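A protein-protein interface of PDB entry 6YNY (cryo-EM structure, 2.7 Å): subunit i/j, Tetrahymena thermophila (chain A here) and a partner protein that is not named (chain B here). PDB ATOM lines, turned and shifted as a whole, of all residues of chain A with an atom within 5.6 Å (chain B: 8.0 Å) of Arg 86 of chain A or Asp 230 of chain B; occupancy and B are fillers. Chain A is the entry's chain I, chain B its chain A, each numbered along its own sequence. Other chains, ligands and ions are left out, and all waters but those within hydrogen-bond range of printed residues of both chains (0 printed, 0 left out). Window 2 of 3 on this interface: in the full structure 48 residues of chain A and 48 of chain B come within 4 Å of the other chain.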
ATOM      1  N   TYR A  71     -11.101  13.658 -15.794  1.00  0.00           N
ATOM      2  CA  TYR A  71     -11.363  15.029 -16.201  1.00  0.00           C
ATOM      3  C   TYR A  71     -12.168  15.750 -15.129  1.00  0.00           C
ATOM      4  O   TYR A  71     -13.050  15.170 -14.493  1.00  0.00           O
ATOM      5  CB  TYR A  71     -12.103  15.064 -17.533  1.00  0.00           C
ATOM      6  CG  TYR A  71     -11.208  14.916 -18.738  1.00  0.00           C
ATOM      7  CD1 TYR A  71     -10.417  15.966 -19.164  1.00  0.00           C
ATOM      8  CD2 TYR A  71     -11.162  13.734 -19.454  1.00  0.00           C
ATOM      9  CE1 TYR A  71      -9.601  15.842 -20.260  1.00  0.00           C
ATOM     10  CE2 TYR A  71     -10.349  13.601 -20.552  1.00  0.00           C
ATOM     11  CZ  TYR A  71      -9.571  14.658 -20.952  1.00  0.00           C
ATOM     12  OH  TYR A  71      -8.760  14.529 -22.049  1.00  0.00           O
ATOM     13  N   SER A  72     -11.861  17.028 -14.941  1.00  0.00           N
ATOM     14  CA  SER A  72     -12.416  17.788 -13.833  1.00  0.00           C
ATOM     15  C   SER A  72     -13.902  18.055 -14.021  1.00  0.00           C
ATOM     16  O   SER A  72     -14.372  18.318 -15.131  1.00  0.00           O
ATOM     17  CB  SER A  72     -11.673  19.111 -13.686  1.00  0.00           C
ATOM     18  OG  SER A  72     -12.253  19.917 -12.679  1.00  0.00           O
ATOM     19  N   PHE A  73     -14.642  17.975 -12.915  1.00  0.00           N
ATOM     20  CA  PHE A  73     -16.037  18.393 -12.910  1.00  0.00           C
ATOM     21  C   PHE A  73     -16.163  19.908 -12.952  1.00  0.00           C
ATOM     22  O   PHE A  73     -17.137  20.433 -13.500  1.00  0.00           O
ATOM     23  CB  PHE A  73     -16.731  17.832 -11.671  1.00  0.00           C
ATOM     24  CG  PHE A  73     -18.043  18.481 -11.355  1.00  0.00           C
ATOM     25  CD1 PHE A  73     -19.209  18.020 -11.926  1.00  0.00           C
ATOM     26  CD2 PHE A  73     -18.113  19.538 -10.471  1.00  0.00           C
ATOM     27  CE1 PHE A  73     -20.414  18.609 -11.631  1.00  0.00           C
ATOM     28  CE2 PHE A  73     -19.316  20.130 -10.177  1.00  0.00           C
ATOM     29  CZ  PHE A  73     -20.467  19.664 -10.758  1.00  0.00           C
ATOM     30  N   SER A  76     -15.610  21.453 -16.594  1.00  0.00           N
ATOM     31  CA  SER A  76     -16.662  21.144 -17.549  1.00  0.00           C
ATOM     32  C   SER A  76     -17.889  22.030 -17.396  1.00  0.00           C
ATOM     33  O   SER A  76     -18.804  21.939 -18.220  1.00  0.00           O
ATOM     34  CB  SER A  76     -17.074  19.682 -17.402  1.00  0.00           C
ATOM     35  OG  SER A  76     -17.669  19.452 -16.141  1.00  0.00           O
ATOM     36  N   HIS A  83     -15.302  20.009 -22.959  1.00  0.00           N
ATOM     37  CA  HIS A  83     -16.515  19.363 -22.465  1.00  0.00           C
ATOM     38  C   HIS A  83     -17.685  20.323 -22.598  1.00  0.00           C
ATOM     39  O   HIS A  83     -17.781  21.300 -21.850  1.00  0.00           O
ATOM     40  CB  HIS A  83     -16.344  18.910 -21.018  1.00  0.00           C
ATOM     41  CG  HIS A  83     -15.761  17.539 -20.874  1.00  0.00           C
ATOM     42  ND1 HIS A  83     -15.014  17.164 -19.779  1.00  0.00           N
ATOM     43  CD2 HIS A  83     -15.835  16.447 -21.669  1.00  0.00           C
ATOM     44  CE1 HIS A  83     -14.640  15.905 -19.915  1.00  0.00           C
ATOM     45  NE2 HIS A  83     -15.127  15.446 -21.052  1.00  0.00           N
ATOM     46  N   MET A  84     -18.565  20.038 -23.555  1.00  0.00           N
ATOM     47  CA  MET A  84     -19.822  20.755 -23.704  1.00  0.00           C
ATOM     48  C   MET A  84     -20.961  20.014 -23.012  1.00  0.00           C
ATOM     49  O   MET A  84     -21.581  20.543 -22.087  1.00  0.00           O
ATOM     50  CB  MET A  84     -20.129  20.947 -25.192  1.00  0.00           C
ATOM     51  CG  MET A  84     -21.390  21.735 -25.480  1.00  0.00           C
ATOM     52  SD  MET A  84     -21.268  23.459 -25.001  1.00  0.00           S
ATOM     53  CE  MET A  84     -20.109  24.025 -26.232  1.00  0.00           C
ATOM     54  N   LEU A  85     -21.231  18.782 -23.433  1.00  0.00           N
ATOM     55  CA  LEU A  85     -22.299  17.963 -22.873  1.00  0.00           C
ATOM     56  C   LEU A  85     -21.674  16.802 -22.116  1.00  0.00           C
ATOM     57  O   LEU A  85     -21.125  15.881 -22.727  1.00  0.00           O
ATOM     58  CB  LEU A  85     -23.232  17.454 -23.965  1.00  0.00           C
ATOM     59  CG  LEU A  85     -24.528  18.228 -24.193  1.00  0.00           C
ATOM     60  CD1 LEU A  85     -24.256  19.606 -24.734  1.00  0.00           C
ATOM     61  CD2 LEU A  85     -25.424  17.463 -25.129  1.00  0.00           C
ATOM     62  N   ARG A  86     -21.761  16.845 -20.790  1.00  0.00           N
ATOM     63  CA  ARG A  86     -21.295  15.763 -19.926  1.00  0.00           C
ATOM     64  C   ARG A  86     -22.387  15.524 -18.891  1.00  0.00           C
ATOM     65  O   ARG A  86     -22.384  16.127 -17.816  1.00  0.00           O
ATOM     66  CB  ARG A  86     -19.960  16.105 -19.286  1.00  0.00           C
ATOM     67  CG  ARG A  86     -19.233  14.904 -18.727  1.00  0.00           C
ATOM     68  CD  ARG A  86     -17.746  15.008 -18.942  1.00  0.00           C
ATOM     69  NE  ARG A  86     -17.098  15.912 -18.001  1.00  0.00           N
ATOM     70  CZ  ARG A  86     -16.362  15.523 -16.963  1.00  0.00           C
ATOM     71  NH1 ARG A  86     -16.163  14.239 -16.710  1.00  0.00           N
ATOM     72  NH2 ARG A  86     -15.811  16.430 -16.174  1.00  0.00           N
ATOM     73  N   VAL A  87     -23.327  14.637 -19.224  1.00  0.00           N
ATOM     74  CA  VAL A  87     -24.471  14.392 -18.358  1.00  0.00           C
ATOM     75  C   VAL A  87     -24.115  13.586 -17.120  1.00  0.00           C
ATOM     76  O   VAL A  87     -24.940  13.479 -16.206  1.00  0.00           O
ATOM     77  CB  VAL A  87     -25.589  13.681 -19.146  1.00  0.00           C
ATOM     78  CG1 VAL A  87     -25.995  14.511 -20.337  1.00  0.00           C
ATOM     79  CG2 VAL A  87     -25.145  12.304 -19.588  1.00  0.00           C
ATOM     80  N   PHE A  88     -22.916  13.015 -17.065  1.00  0.00           N
ATOM     81  CA  PHE A  88     -22.425  12.309 -15.890  1.00  0.00           C
ATOM     82  C   PHE A  88     -21.139  12.940 -15.375  1.00  0.00           C
ATOM     83  O   PHE A  88     -20.216  12.251 -14.940  1.00  0.00           O
ATOM     84  CB  PHE A  88     -22.216  10.827 -16.183  1.00  0.00           C
ATOM     85  CG  PHE A  88     -23.488  10.046 -16.295  1.00  0.00           C
ATOM     86  CD1 PHE A  88     -24.300   9.857 -15.193  1.00  0.00           C
ATOM     87  CD2 PHE A  88     -23.867   9.491 -17.500  1.00  0.00           C
ATOM     88  CE1 PHE A  88     -25.469   9.139 -15.295  1.00  0.00           C
ATOM     89  CE2 PHE A  88     -25.033   8.771 -17.605  1.00  0.00           C
ATOM     90  CZ  PHE A  88     -25.834   8.594 -16.501  1.00  0.00           C
ATOM     91  N   ARG A  89     -21.069  14.270 -15.416  1.00  0.00           N
ATOM     92  CA  ARG A  89     -19.923  14.962 -14.844  1.00  0.00           C
ATOM     93  C   ARG A  89     -19.917  14.874 -13.324  1.00  0.00           C
ATOM     94  O   ARG A  89     -18.849  14.926 -12.706  1.00  0.00           O
ATOM     95  CB  ARG A  89     -19.915  16.425 -15.288  1.00  0.00           C
ATOM     96  CG  ARG A  89     -21.194  17.168 -14.982  1.00  0.00           C
ATOM     97  CD  ARG A  89     -21.018  18.668 -15.071  1.00  0.00           C
ATOM     98  NE  ARG A  89     -20.493  19.114 -16.357  1.00  0.00           N
ATOM     99  CZ  ARG A  89     -21.236  19.384 -17.424  1.00  0.00           C
ATOM    100  NH1 ARG A  89     -22.551  19.250 -17.385  1.00  0.00           N
ATOM    101  NH2 ARG A  89     -20.658  19.787 -18.540  1.00  0.00           N
ATOM    102  N   HIS A  90     -21.090  14.740 -12.708  1.00  0.00           N
ATOM    103  CA  HIS A  90     -21.187  14.608 -11.259  1.00  0.00           C
ATOM    104  C   HIS A  90     -20.687  13.266 -10.742  1.00  0.00           C
ATOM    105  O   HIS A  90     -20.762  13.028  -9.531  1.00  0.00           O
ATOM    106  CB  HIS A  90     -22.628  14.842 -10.799  1.00  0.00           C
ATOM    107  CG  HIS A  90     -23.629  13.890 -11.380  1.00  0.00           C
ATOM    108  ND1 HIS A  90     -23.451  13.256 -12.591  1.00  0.00           N
ATOM    109  CD2 HIS A  90     -24.830  13.476 -10.915  1.00  0.00           C
ATOM    110  CE1 HIS A  90     -24.498  12.493 -12.844  1.00  0.00           C
ATOM    111  NE2 HIS A  90     -25.348  12.608 -11.842  1.00  0.00           N
ATOM    112  N   PHE A  91     -20.190  12.388 -11.609  1.00  0.00           N
ATOM    113  CA  PHE A  91     -19.556  11.144 -11.204  1.00  0.00           C
ATOM    114  C   PHE A  91     -18.039  11.207 -11.329  1.00  0.00           C
ATOM    115  O   PHE A  91     -17.364  10.193 -11.134  1.00  0.00           O
ATOM    116  CB  PHE A  91     -20.109   9.989 -12.040  1.00  0.00           C
ATOM    117  CG  PHE A  91     -19.782   8.633 -11.498  1.00  0.00           C
ATOM    118  CD1 PHE A  91     -20.531   8.081 -10.478  1.00  0.00           C
ATOM    119  CD2 PHE A  91     -18.731   7.903 -12.016  1.00  0.00           C
ATOM    120  CE1 PHE A  91     -20.231   6.835  -9.983  1.00  0.00           C
ATOM    121  CE2 PHE A  91     -18.427   6.660 -11.521  1.00  0.00           C
ATOM    122  CZ  PHE A  91     -19.178   6.124 -10.505  1.00  0.00           C
ATOM    123  N   ALA A  92     -17.488  12.384 -11.626  1.00  0.00           N
ATOM    124  CA  ALA A  92     -16.063  12.490 -11.919  1.00  0.00           C
ATOM    125  C   ALA A  92     -15.199  12.220 -10.693  1.00  0.00           C
ATOM    126  O   ALA A  92     -14.141  11.592 -10.806  1.00  0.00           O
ATOM    127  CB  ALA A  92     -15.756  13.873 -12.487  1.00  0.00           C
ATOM    128  N   ILE B 225     -23.861   7.183 -26.075  1.00  0.00           N
ATOM    129  CA  ILE B 225     -24.605   7.547 -24.876  1.00  0.00           C
ATOM    130  C   ILE B 225     -23.977   8.770 -24.222  1.00  0.00           C
ATOM    131  O   ILE B 225     -24.587   9.842 -24.138  1.00  0.00           O
ATOM    132  CB  ILE B 225     -24.654   6.358 -23.900  1.00  0.00           C
ATOM    133  CG1 ILE B 225     -25.266   5.127 -24.569  1.00  0.00           C
ATOM    134  CG2 ILE B 225     -25.419   6.722 -22.652  1.00  0.00           C
ATOM    135  CD1 ILE B 225     -26.670   5.318 -25.066  1.00  0.00           C
ATOM    136  N   THR B 226     -22.749   8.620 -23.753  1.00  0.00           N
ATOM    137  CA  THR B 226     -21.938   9.704 -23.210  1.00  0.00           C
ATOM    138  C   THR B 226     -20.537   9.139 -23.011  1.00  0.00           C
ATOM    139  O   THR B 226     -20.240   8.017 -23.439  1.00  0.00           O
ATOM    140  CB  THR B 226     -22.531  10.276 -21.920  1.00  0.00           C
ATOM    141  OG1 THR B 226     -21.681  11.315 -21.419  1.00  0.00           O
ATOM    142  CG2 THR B 226     -22.681   9.205 -20.857  1.00  0.00           C
ATOM    143  N   SER B 227     -19.670   9.916 -22.375  1.00  0.00           N
ATOM    144  CA  SER B 227     -18.308   9.471 -22.122  1.00  0.00           C
ATOM    145  C   SER B 227     -18.307   8.140 -21.385  1.00  0.00           C
ATOM    146  O   SER B 227     -18.771   8.049 -20.245  1.00  0.00           O
ATOM    147  CB  SER B 227     -17.557  10.526 -21.310  1.00  0.00           C
ATOM    148  OG  SER B 227     -17.488  11.755 -22.006  1.00  0.00           O
ATOM    149  N   ILE B 228     -17.789   7.102 -22.044  1.00  0.00           N
ATOM    150  CA  ILE B 228     -17.681   5.797 -21.403  1.00  0.00           C
ATOM    151  C   ILE B 228     -16.752   5.869 -20.206  1.00  0.00           C
ATOM    152  O   ILE B 228     -16.868   5.061 -19.281  1.00  0.00           O
ATOM    153  CB  ILE B 228     -17.214   4.735 -22.424  1.00  0.00           C
ATOM    154  CG1 ILE B 228     -17.122   3.347 -21.791  1.00  0.00           C
ATOM    155  CG2 ILE B 228     -15.872   5.085 -22.993  1.00  0.00           C
ATOM    156  CD1 ILE B 228     -18.440   2.770 -21.361  1.00  0.00           C
ATOM    157  N   ASP B 229     -15.829   6.830 -20.197  1.00  0.00           N
ATOM    158  CA  ASP B 229     -14.943   7.009 -19.057  1.00  0.00           C
ATOM    159  C   ASP B 229     -15.688   7.510 -17.831  1.00  0.00           C
ATOM    160  O   ASP B 229     -15.179   7.381 -16.713  1.00  0.00           O
ATOM    161  CB  ASP B 229     -13.823   7.980 -19.426  1.00  0.00           C
ATOM    162  CG  ASP B 229     -12.774   8.101 -18.347  1.00  0.00           C
ATOM    163  OD1 ASP B 229     -12.065   7.106 -18.091  1.00  0.00           O
ATOM    164  OD2 ASP B 229     -12.648   9.197 -17.765  1.00  0.00           O
ATOM    165  N   ASP B 230     -16.880   8.073 -18.013  1.00  0.00           N
ATOM    166  CA  ASP B 230     -17.671   8.591 -16.909  1.00  0.00           C
ATOM    167  C   ASP B 230     -18.634   7.548 -16.353  1.00  0.00           C
ATOM    168  O   ASP B 230     -18.654   7.305 -15.144  1.00  0.00           O
ATOM    169  CB  ASP B 230     -18.452   9.826 -17.355  1.00  0.00           C
ATOM    170  CG  ASP B 230     -17.567  11.033 -17.560  1.00  0.00           C
ATOM    171  OD1 ASP B 230     -16.340  10.917 -17.363  1.00  0.00           O
ATOM    172  OD2 ASP B 230     -18.103  12.101 -17.914  1.00  0.00           O
ATOM    173  N   TYR B 231     -19.435   6.930 -17.215  1.00  0.00           N
ATOM    174  CA  TYR B 231     -20.511   6.064 -16.759  1.00  0.00           C
ATOM    175  C   TYR B 231     -20.099   4.608 -16.620  1.00  0.00           C
ATOM    176  O   TYR B 231     -20.932   3.780 -16.242  1.00  0.00           O
ATOM    177  CB  TYR B 231     -21.716   6.176 -17.702  1.00  0.00           C
ATOM    178  CG  TYR B 231     -21.577   5.489 -19.043  1.00  0.00           C
ATOM    179  CD1 TYR B 231     -21.759   4.122 -19.171  1.00  0.00           C
ATOM    180  CD2 TYR B 231     -21.311   6.217 -20.188  1.00  0.00           C
ATOM    181  CE1 TYR B 231     -21.648   3.500 -20.390  1.00  0.00           C
ATOM    182  CE2 TYR B 231     -21.203   5.603 -21.413  1.00  0.00           C
ATOM    183  CZ  TYR B 231     -21.372   4.246 -21.510  1.00  0.00           C
ATOM    184  OH  TYR B 231     -21.262   3.633 -22.734  1.00  0.00           O
ATOM    185  N   LEU B 232     -18.844   4.267 -16.912  1.00  0.00           N
ATOM    186  CA  LEU B 232     -18.417   2.884 -16.745  1.00  0.00           C
ATOM    187  C   LEU B 232     -18.406   2.482 -15.277  1.00  0.00           C
ATOM    188  O   LEU B 232     -18.621   1.309 -14.955  1.00  0.00           O
ATOM    189  CB  LEU B 232     -17.041   2.676 -17.367  1.00  0.00           C
ATOM    190  CG  LEU B 232     -16.489   1.253 -17.319  1.00  0.00           C
ATOM    191  CD1 LEU B 232     -17.419   0.304 -18.038  1.00  0.00           C
ATOM    192  CD2 LEU B 232     -15.107   1.195 -17.922  1.00  0.00           C
ATOM    193  N   GLY B 233     -18.155   3.436 -14.380  1.00  0.00           N
ATOM    194  CA  GLY B 233     -18.202   3.142 -12.960  1.00  0.00           C
ATOM    195  C   GLY B 233     -19.605   2.900 -12.448  1.00  0.00           C
ATOM    196  O   GLY B 233     -19.803   2.100 -11.530  1.00  0.00           O
ATOM    197  N   LEU B 234     -20.594   3.582 -13.025  1.00  0.00           N
ATOM    198  CA  LEU B 234     -21.978   3.344 -12.634  1.00  0.00           C
ATOM    199  C   LEU B 234     -22.462   1.984 -13.109  1.00  0.00           C
ATOM    200  O   LEU B 234     -23.298   1.360 -12.448  1.00  0.00           O
ATOM    201  CB  LEU B 234     -22.875   4.446 -13.186  1.00  0.00           C
ATOM    202  CG  LEU B 234     -22.717   5.824 -12.551  1.00  0.00           C
ATOM    203  CD1 LEU B 234     -23.473   6.866 -13.352  1.00  0.00           C
ATOM    204  CD2 LEU B 234     -23.197   5.803 -11.113  1.00  0.00           C
ATOM    205  N   VAL B 235     -21.952   1.508 -14.245  1.00  0.00           N
ATOM    206  CA  VAL B 235     -22.309   0.176 -14.716  1.00  0.00           C
ATOM    207  C   VAL B 235     -21.889  -0.871 -13.696  1.00  0.00           C
ATOM    208  O   VAL B 235     -22.614  -1.839 -13.441  1.00  0.00           O
ATOM    209  CB  VAL B 235     -21.673  -0.088 -16.091  1.00  0.00           C
ATOM    210  CG1 VAL B 235     -21.849  -1.529 -16.492  1.00  0.00           C
ATOM    211  CG2 VAL B 235     -22.275   0.823 -17.128  1.00  0.00           C
ATOM    212  N   GLY B 276     -29.870  12.894 -11.559  1.00  0.00           N
ATOM    213  CA  GLY B 276     -29.119  14.083 -11.893  1.00  0.00           C
ATOM    214  C   GLY B 276     -28.785  14.208 -13.362  1.00  0.00           C
ATOM    215  O   GLY B 276     -28.463  15.300 -13.835  1.00  0.00           O
ATOM    216  N   MET B 277     -28.855  13.101 -14.097  1.00  0.00           N
ATOM    217  CA  MET B 277     -28.565  13.159 -15.525  1.00  0.00           C
ATOM    218  C   MET B 277     -29.471  14.138 -16.255  1.00  0.00           C
ATOM    219  O   MET B 277     -28.961  14.902 -17.094  1.00  0.00           O
ATOM    220  CB  MET B 277     -28.673  11.755 -16.128  1.00  0.00           C
ATOM    221  CG  MET B 277     -28.151  11.645 -17.545  1.00  0.00           C
ATOM    222  SD  MET B 277     -28.380  10.016 -18.273  1.00  0.00           S
ATOM    223  CE  MET B 277     -30.162   9.920 -18.300  1.00  0.00           C
ATOM    224  N   LEU B 280     -28.369  17.941 -15.118  1.00  0.00           N
ATOM    225  CA  LEU B 280     -27.175  18.487 -15.752  1.00  0.00           C
ATOM    226  C   LEU B 280     -27.388  18.717 -17.240  1.00  0.00           C
ATOM    227  O   LEU B 280     -26.751  19.596 -17.828  1.00  0.00           O
ATOM    228  CB  LEU B 280     -25.986  17.554 -15.537  1.00  0.00           C
ATOM    229  CG  LEU B 280     -25.243  17.610 -14.201  1.00  0.00           C
ATOM    230  CD1 LEU B 280     -24.724  19.010 -13.906  1.00  0.00           C
ATOM    231  CD2 LEU B 280     -26.116  17.120 -13.077  1.00  0.00           C
ATOM    232  N   LEU B 281     -28.274  17.942 -17.863  1.00  0.00           N
ATOM    233  CA  LEU B 281     -28.553  18.135 -19.281  1.00  0.00           C
ATOM    234  C   LEU B 281     -29.225  19.477 -19.529  1.00  0.00           C
ATOM    235  O   LEU B 281     -28.923  20.154 -20.516  1.00  0.00           O
ATOM    236  CB  LEU B 281     -29.419  16.991 -19.799  1.00  0.00           C
ATOM    237  CG  LEU B 281     -29.763  17.019 -21.283  1.00  0.00           C
ATOM    238  CD1 LEU B 281     -28.505  17.075 -22.108  1.00  0.00           C
ATOM    239  CD2 LEU B 281     -30.582  15.809 -21.655  1.00  0.00           C
ATOM    240  N   TYR B 283     -28.820  22.076 -17.516  1.00  0.00           N
ATOM    241  CA  TYR B 283     -27.744  23.026 -17.276  1.00  0.00           C
ATOM    242  C   TYR B 283     -26.866  23.187 -18.506  1.00  0.00           C
ATOM    243  O   TYR B 283     -26.308  24.266 -18.733  1.00  0.00           O
ATOM    244  CB  TYR B 283     -26.912  22.574 -16.077  1.00  0.00           C
ATOM    245  CG  TYR B 283     -25.647  23.367 -15.870  1.00  0.00           C
ATOM    246  CD1 TYR B 283     -24.428  22.897 -16.326  1.00  0.00           C
ATOM    247  CD2 TYR B 283     -25.671  24.586 -15.217  1.00  0.00           C
ATOM    248  CE1 TYR B 283     -23.276  23.617 -16.139  1.00  0.00           C
ATOM    249  CE2 TYR B 283     -24.525  25.312 -15.027  1.00  0.00           C
ATOM    250  CZ  TYR B 283     -23.328  24.825 -15.486  1.00  0.00           C
ATOM    251  OH  TYR B 283     -22.180  25.553 -15.297  1.00  0.00           O
ATOM    252  N   ASP B 284     -26.732  22.134 -19.312  1.00  0.00           N
ATOM    253  CA  ASP B 284     -25.939  22.235 -20.527  1.00  0.00           C
ATOM    254  C   ASP B 284     -26.671  23.002 -21.617  1.00  0.00           C
ATOM    255  O   ASP B 284     -26.033  23.686 -22.423  1.00  0.00           O
ATOM    256  CB  ASP B 284     -25.561  20.842 -21.033  1.00  0.00           C
ATOM    257  CG  ASP B 284     -24.605  20.121 -20.104  1.00  0.00           C
ATOM    258  OD1 ASP B 284     -23.840  20.800 -19.391  1.00  0.00           O
ATOM    259  OD2 ASP B 284     -24.614  18.873 -20.092  1.00  0.00           O
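Of the 17 printed residues of chain B, 8 touch a printed residue of chain A. Hydrophobic or aromatic side chains of chain B within 4 Å of the printed part of chain A: Tyr 231, Leu 234, Met 277 and Leu 280. Along chain B the printed residues that touch a printed residue of chain A span positions 226 to 284. Among the printed residues, Asp or Glu carboxylates within 4 Å of a Lys or Arg side-chain nitrogen of the other chain: Arg 86 of chain A with Asp 230 of chain B and Arg 89 of chain A with Asp 284 of chain B.
The side-chain carboxylate (OD2) of Asp 230 of chain B lies within salt-bridge range of the guanidinium group (NH1) of Arg 86 of chain A. The side-chain carboxylate of Asp 284 of chain B is in salt-bridge range of the guanidinium group of Arg 89 of chain A.
Arg 86 of chain A touches just these residues of chain B: Asp 230 and Asp 284. Of chain A, only Arg 86 (3.1 Å), Phe 88 (3.7 Å) and Phe 91 (3.2 Å) come within 4 Å of Asp 230 of chain B. Printed residues of chain B within 4 Å of Phe 91 of chain A: Asp 230 (3.2 Å), Gly 233 (3.8 Å) and Leu 234 (3.3 Å). Printed residues of chain A within 4 Å of Leu 280 of chain B: Arg 89 (3.9 Å). Of the printed residues of chain A, Leu 234 of chain B touches Phe 88 (3.6 Å) and Phe 91 (3.3 Å). Printed residues of chain A within 4 Å of Gly 233 of chain B: Phe 91 (3.8 Å). Of the printed residues of chain B, Leu 85 of chain A touches Asp 284. His 90 of chain A touches none of the printed residues of chain B. The nearest printed residue of chain B that does not touch Arg 86 of chain A is Ser 227 of chain B (4.5 Å).
O of Tyr 71 of chain A lies within hydrogen-bond range of NH2 of Arg 86 of chain A, 3.5 Å away. O of Ser 72 of chain A lies within hydrogen-bond range of NH2 of Arg 86 of chain A. NE of Arg 89 of chain A is in hydrogen-bond range of OG of Ser 76 of chain A, at 2.9 Å. The guanidinium group of Arg 86 of chain A is in hydrogen-bond range of a ring nitrogen (ND1) of His 83 of chain A, at 3.0 Å. NH1 of Arg 89 of chain A is in hydrogen-bond range of O of Arg 86 of chain A (3.2 Å).
Among the printed residues, merely in contact across the chains: Met 84 of chain A with Asp 284 of chain B (3.5 Å), Leu 85 of chain A with Asp 284 of chain B (3.7 Å), Arg 86 of chain A with Asp 284 of chain B (3.6 Å), Val 87 of chain A with Met 277 of chain B (3.6 Å), Phe 88 of chain A with Thr 226 of chain B (3.6 Å), Phe 88 of chain A with Asp 230 of chain B (3.7 Å), Phe 88 of chain A with Tyr 231 of chain B (3.96 Å), Phe 88 of chain A with Leu 234 of chain B (3.6 Å), Phe 88 of chain A with Met 277 of chain B (3.4 Å), Arg 89 of chain A with Leu 280 of chain B (3.9 Å), Phe 91 of chain A with Asp 230 of chain B (3.2 Å), Phe 91 of chain A with Gly 233 of chain B (3.8 Å) and Phe 91 of chain A with Leu 234 of chain B (3.3 Å).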
